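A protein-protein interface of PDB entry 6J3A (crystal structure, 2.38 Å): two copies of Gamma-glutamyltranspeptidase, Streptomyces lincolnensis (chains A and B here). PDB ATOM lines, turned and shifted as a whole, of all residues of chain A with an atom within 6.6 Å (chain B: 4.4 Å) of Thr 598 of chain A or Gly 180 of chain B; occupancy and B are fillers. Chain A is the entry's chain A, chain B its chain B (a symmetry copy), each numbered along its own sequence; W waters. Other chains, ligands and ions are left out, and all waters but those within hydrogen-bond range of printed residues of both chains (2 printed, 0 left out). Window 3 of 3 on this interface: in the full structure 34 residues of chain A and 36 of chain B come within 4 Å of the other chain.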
ATOM      1  N   GLN A   9       0.810   7.073 -17.701  1.00  0.00           N
ATOM      2  CA  GLN A   9      -0.451   6.788 -17.014  1.00  0.00           C
ATOM      3  C   GLN A   9      -0.179   6.480 -15.552  1.00  0.00           C
ATOM      4  O   GLN A   9       0.769   5.766 -15.243  1.00  0.00           O
ATOM      5  CB  GLN A   9      -1.121   5.591 -17.655  1.00  0.00           C
ATOM      6  CG  GLN A   9      -1.815   5.923 -18.958  1.00  0.00           C
ATOM      7  CD  GLN A   9      -2.382   4.699 -19.630  1.00  0.00           C
ATOM      8  OE1 GLN A   9      -1.702   3.684 -19.773  1.00  0.00           O
ATOM      9  NE2 GLN A   9      -3.627   4.789 -20.061  1.00  0.00           N
ATOM     10  N   THR A  11      -1.691   7.321 -11.046  1.00  0.00           N
ATOM     11  CA  THR A  11      -2.734   7.606 -10.043  1.00  0.00           C
ATOM     12  C   THR A  11      -2.317   8.526  -8.892  1.00  0.00           C
ATOM     13  O   THR A  11      -3.057   8.666  -7.912  1.00  0.00           O
ATOM     14  CB  THR A  11      -3.214   6.291  -9.395  1.00  0.00           C
ATOM     15  OG1 THR A  11      -2.092   5.600  -8.834  1.00  0.00           O
ATOM     16  CG2 THR A  11      -3.874   5.405 -10.415  1.00  0.00           C
ATOM     17  N   VAL A 523      -5.106   5.218 -27.028  1.00  0.00           N
ATOM     18  CA  VAL A 523      -3.949   4.352 -26.889  1.00  0.00           C
ATOM     19  C   VAL A 523      -3.934   3.944 -25.424  1.00  0.00           C
ATOM     20  O   VAL A 523      -4.059   4.801 -24.539  1.00  0.00           O
ATOM     21  CB  VAL A 523      -2.667   5.100 -27.289  1.00  0.00           C
ATOM     22  CG1 VAL A 523      -1.411   4.303 -26.934  1.00  0.00           C
ATOM     23  CG2 VAL A 523      -2.705   5.424 -28.786  1.00  0.00           C
ATOM     24  N   ARG A 524      -3.826   2.638 -25.179  1.00  0.00           N
ATOM     25  CA  ARG A 524      -3.912   2.072 -23.825  1.00  0.00           C
ATOM     26  C   ARG A 524      -5.159   2.533 -23.088  1.00  0.00           C
ATOM     27  O   ARG A 524      -5.087   2.967 -21.934  1.00  0.00           O
ATOM     28  CB  ARG A 524      -2.656   2.400 -23.005  1.00  0.00           C
ATOM     29  CG  ARG A 524      -1.436   1.681 -23.526  1.00  0.00           C
ATOM     30  CD  ARG A 524      -0.176   2.052 -22.773  1.00  0.00           C
ATOM     31  NE  ARG A 524       0.984   1.396 -23.376  1.00  0.00           N
ATOM     32  CZ  ARG A 524       2.255   1.713 -23.141  1.00  0.00           C
ATOM     33  NH1 ARG A 524       2.575   2.707 -22.299  1.00  0.00           N
ATOM     34  NH2 ARG A 524       3.220   1.032 -23.763  1.00  0.00           N
ATOM     35  N   GLY A 525      -6.302   2.452 -23.768  1.00  0.00           N
ATOM     36  CA  GLY A 525      -7.584   2.914 -23.214  1.00  0.00           C
ATOM     37  C   GLY A 525      -7.624   4.349 -22.688  1.00  0.00           C
ATOM     38  O   GLY A 525      -8.441   4.657 -21.831  1.00  0.00           O
ATOM     39  N   GLY A 526      -6.746   5.216 -23.202  1.00  0.00           N
ATOM     40  CA  GLY A 526      -6.656   6.624 -22.791  1.00  0.00           C
ATOM     41  C   GLY A 526      -6.392   7.523 -23.991  1.00  0.00           C
ATOM     42  O   GLY A 526      -5.984   7.052 -25.056  1.00  0.00           O
ATOM     43  N   ASP A 595      -8.849  10.839 -16.757  1.00  0.00           N
ATOM     44  CA  ASP A 595     -10.036  10.112 -17.183  1.00  0.00           C
ATOM     45  C   ASP A 595     -10.997  10.186 -16.000  1.00  0.00           C
ATOM     46  O   ASP A 595     -10.673   9.692 -14.916  1.00  0.00           O
ATOM     47  CB  ASP A 595      -9.680   8.665 -17.507  1.00  0.00           C
ATOM     48  CG  ASP A 595     -10.873   7.845 -18.011  1.00  0.00           C
ATOM     49  OD1 ASP A 595     -12.043   8.176 -17.728  1.00  0.00           O
ATOM     50  OD2 ASP A 595     -10.623   6.830 -18.683  1.00  0.00           O
ATOM     51  N   PRO A 596     -12.171  10.816 -16.194  1.00  0.00           N
ATOM     52  CA  PRO A 596     -13.110  10.975 -15.070  1.00  0.00           C
ATOM     53  C   PRO A 596     -13.768   9.650 -14.600  1.00  0.00           C
ATOM     54  O   PRO A 596     -13.910   9.435 -13.383  1.00  0.00           O
ATOM     55  CB  PRO A 596     -14.141  11.972 -15.611  1.00  0.00           C
ATOM     56  CG  PRO A 596     -14.090  11.817 -17.094  1.00  0.00           C
ATOM     57  CD  PRO A 596     -12.712  11.355 -17.456  1.00  0.00           C
ATOM     58  N   ARG A 597     -14.141   8.784 -15.553  1.00  0.00           N
ATOM     59  CA  ARG A 597     -14.741   7.464 -15.262  1.00  0.00           C
ATOM     60  C   ARG A 597     -13.877   6.626 -14.312  1.00  0.00           C
ATOM     61  O   ARG A 597     -14.383   6.074 -13.334  1.00  0.00           O
ATOM     62  CB  ARG A 597     -14.995   6.682 -16.556  1.00  0.00           C
ATOM     63  N   THR A 598     -12.572   6.592 -14.587  1.00  0.00           N
ATOM     64  CA  THR A 598     -11.606   5.730 -13.875  1.00  0.00           C
ATOM     65  C   THR A 598     -10.655   6.423 -12.867  1.00  0.00           C
ATOM     66  O   THR A 598     -10.055   5.747 -12.025  1.00  0.00           O
ATOM     67  CB  THR A 598     -10.788   4.896 -14.891  1.00  0.00           C
ATOM     68  OG1 THR A 598     -10.109   3.839 -14.204  1.00  0.00           O
ATOM     69  CG2 THR A 598      -9.783   5.726 -15.620  1.00  0.00           C
ATOM     70  N   GLY A 599     -10.503   7.746 -12.964  1.00  0.00           N
ATOM     71  CA  GLY A 599      -9.619   8.516 -12.065  1.00  0.00           C
ATOM     72  C   GLY A 599      -8.140   8.555 -12.452  1.00  0.00           C
ATOM     73  O   GLY A 599      -7.330   9.194 -11.766  1.00  0.00           O
ATOM     74  N   ILE A 600      -7.803   7.919 -13.573  1.00  0.00           N
ATOM     75  CA  ILE A 600      -6.425   7.707 -14.011  1.00  0.00           C
ATOM     76  C   ILE A 600      -5.895   8.995 -14.624  1.00  0.00           C
ATOM     77  O   ILE A 600      -6.540   9.592 -15.479  1.00  0.00           O
ATOM     78  CB  ILE A 600      -6.321   6.546 -15.039  1.00  0.00           C
ATOM     79  CG1 ILE A 600      -6.474   5.205 -14.317  1.00  0.00           C
ATOM     80  CG2 ILE A 600      -4.993   6.561 -15.807  1.00  0.00           C
ATOM     81  CD1 ILE A 600      -6.772   4.026 -15.222  1.00  0.00           C
ATOM     82  N   LEU A 601      -4.695   9.376 -14.199  1.00  0.00           N
ATOM     83  CA  LEU A 601      -4.004  10.582 -14.655  1.00  0.00           C
ATOM     84  C   LEU A 601      -3.036  10.221 -15.763  1.00  0.00           C
ATOM     85  O   LEU A 601      -2.386   9.175 -15.695  1.00  0.00           O
ATOM     86  CB  LEU A 601      -3.229  11.177 -13.487  1.00  0.00           C
ATOM     87  CG  LEU A 601      -4.031  11.346 -12.203  1.00  0.00           C
ATOM     88  CD1 LEU A 601      -3.187  11.958 -11.108  1.00  0.00           C
ATOM     89  CD2 LEU A 601      -5.252  12.207 -12.458  1.00  0.00           C
ATOM     90  N   ALA B 143      -2.639   1.478 -14.242  1.00  0.00           N
ATOM     91  CA  ALA B 143      -3.063   1.256 -15.614  1.00  0.00           C
ATOM     92  C   ALA B 143      -1.967   0.505 -16.344  1.00  0.00           C
ATOM     93  O   ALA B 143      -0.907   1.071 -16.607  1.00  0.00           O
ATOM     94  CB  ALA B 143      -3.347   2.579 -16.296  1.00  0.00           C
ATOM     95  N   ARG B 178      -6.795  -5.098 -18.571  1.00  0.00           N
ATOM     96  CA  ARG B 178      -7.068  -4.219 -19.717  1.00  0.00           C
ATOM     97  C   ARG B 178      -6.296  -2.929 -19.504  1.00  0.00           C
ATOM     98  O   ARG B 178      -6.311  -2.375 -18.393  1.00  0.00           O
ATOM     99  CB  ARG B 178      -8.573  -3.892 -19.908  1.00  0.00           C
ATOM    100  CG  ARG B 178      -9.566  -4.945 -19.418  1.00  0.00           C
ATOM    101  CD  ARG B 178     -10.512  -5.491 -20.494  1.00  0.00           C
ATOM    102  NE  ARG B 178     -10.657  -6.959 -20.391  1.00  0.00           N
ATOM    103  CZ  ARG B 178     -11.349  -7.746 -21.224  1.00  0.00           C
ATOM    104  NH1 ARG B 178     -12.003  -7.239 -22.270  1.00  0.00           N
ATOM    105  NH2 ARG B 178     -11.386  -9.063 -21.011  1.00  0.00           N
ATOM    106  N   PRO B 179      -5.621  -2.441 -20.554  1.00  0.00           N
ATOM    107  CA  PRO B 179      -5.067  -1.109 -20.415  1.00  0.00           C
ATOM    108  C   PRO B 179      -6.178  -0.056 -20.232  1.00  0.00           C
ATOM    109  O   PRO B 179      -7.322  -0.249 -20.661  1.00  0.00           O
ATOM    110  CB  PRO B 179      -4.291  -0.906 -21.716  1.00  0.00           C
ATOM    111  CG  PRO B 179      -4.872  -1.862 -22.690  1.00  0.00           C
ATOM    112  CD  PRO B 179      -5.374  -3.018 -21.890  1.00  0.00           C
ATOM    113  N   GLY B 180      -5.841   1.021 -19.536  1.00  0.00           N
ATOM    114  CA  GLY B 180      -6.810   2.059 -19.209  1.00  0.00           C
ATOM    115  C   GLY B 180      -7.683   1.756 -18.007  1.00  0.00           C
ATOM    116  O   GLY B 180      -8.456   2.607 -17.597  1.00  0.00           O
ATOM    117  N   GLU B 181      -7.585   0.552 -17.450  1.00  0.00           N
ATOM    118  CA  GLU B 181      -8.316   0.197 -16.233  1.00  0.00           C
ATOM    119  C   GLU B 181      -7.333  -0.168 -15.137  1.00  0.00           C
ATOM    120  O   GLU B 181      -6.242  -0.677 -15.415  1.00  0.00           O
ATOM    121  CB  GLU B 181      -9.283  -0.968 -16.491  1.00  0.00           C
ATOM    122  CG  GLU B 181     -10.761  -0.584 -16.498  1.00  0.00           C
ATOM    123  CD  GLU B 181     -11.347  -0.517 -17.891  1.00  0.00           C
ATOM    124  OE1 GLU B 181     -11.517  -1.587 -18.516  1.00  0.00           O
ATOM    125  OE2 GLU B 181     -11.652   0.600 -18.353  1.00  0.00           O
ATOM    126  N   LEU B 182      -7.721   0.087 -13.892  1.00  0.00           N
ATOM    127  CA  LEU B 182      -6.878  -0.246 -12.749  1.00  0.00           C
ATOM    128  C   LEU B 182      -6.733  -1.758 -12.530  1.00  0.00           C
ATOM    129  O   LEU B 182      -7.682  -2.420 -12.123  1.00  0.00           O
ATOM    130  CB  LEU B 182      -7.421   0.401 -11.473  1.00  0.00           C
ATOM    131  CG  LEU B 182      -7.449   1.936 -11.446  1.00  0.00           C
ATOM    132  CD1 LEU B 182      -8.038   2.441 -10.130  1.00  0.00           C
ATOM    133  CD2 LEU B 182      -6.066   2.542 -11.670  1.00  0.00           C
HETATM  134  O   HOH W   1      -3.003   1.535 -19.212  1.00  0.00           O
HETATM  135  O   HOH W   2      -0.518   3.267 -14.562  1.00  0.00           O
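N of Gly 180 of chain B lies within hydrogen-bond range of O of Arg 524 of chain A (3.2 Å).
The backbone NH (N) of Asp 595 of chain A lies within hydrogen-bond range of the backbone carbonyl oxygen (O) of Ile 600 of chain A, at 2.9 Å. O of Arg 524 of chain A is in hydrogen-bond range of NE2 of Gln 9 of chain A.
Gln 9 of chain A touches Ala 143 of chain B (CB to CB, 3.98 Å). Thr 11 of chain A touches Leu 182 of chain B. Arg 524 of chain A touches Pro 179 of chain B. Gly 180 of chain B touches Thr 598 of chain A. Ile 600 of chain A touches Ala 143 of chain B. Ile 600 of chain A touches Gly 180 of chain B (CD1 to O, 3.2 Å). Leu 182 of chain B touches Ile 600 of chain A.
Printed residues of chain B within 4 Å of Thr 11 of chain A: Leu 182 (3.8 Å). Printed residues of chain B within 4 Å of Arg 524 of chain A: Pro 179 and Gly 180. Of chain B, only Gly 180 (3.9 Å) comes within 4 Å of Thr 598 of chain A. Gly 180 of chain B touches just these residues of chain A: Arg 524 (3.2 Å), Thr 598 (3.9 Å) and Ile 600 (3.2 Å). Printed residues of chain A within 4 Å of Leu 182 of chain B: Thr 11 and Ile 600. The nearest residue of chain B that does not touch Thr 598 of chain A is Leu 182 of chain B (4.3 Å).
Of the 6 printed residues of chain B, 4 touch a printed residue of chain A. Hydrophobic or aromatic side chains of chain B that line the printed part of chain A: Ala 143, Pro 179 and Leu 182. Among the printed residues, 8 pairs touch across the chains. Among the printed residues, no Asp or Glu carboxylate lies within 4 Å of a Lys or Arg side-chain nitrogen of the other chain.
No position is printed for both chains. Of the 8 pairs that touch across the chains among the printed residues, none has its exchanged pair printed and touching as well.
Water W1 lies within hydrogen-bond range of the side-chain amide oxygen (OE1) of Gln 9 of chain A (2.6 Å), the backbone NH (N) of Gly 180 of chain B (2.9 Å) and the backbone carbonyl oxygen (O) of Ala 143 of chain B (3.4 Å). Water W2 lies within hydrogen-bond range of N of Ala 143 of chain B and O of Gln 9 of chain A.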
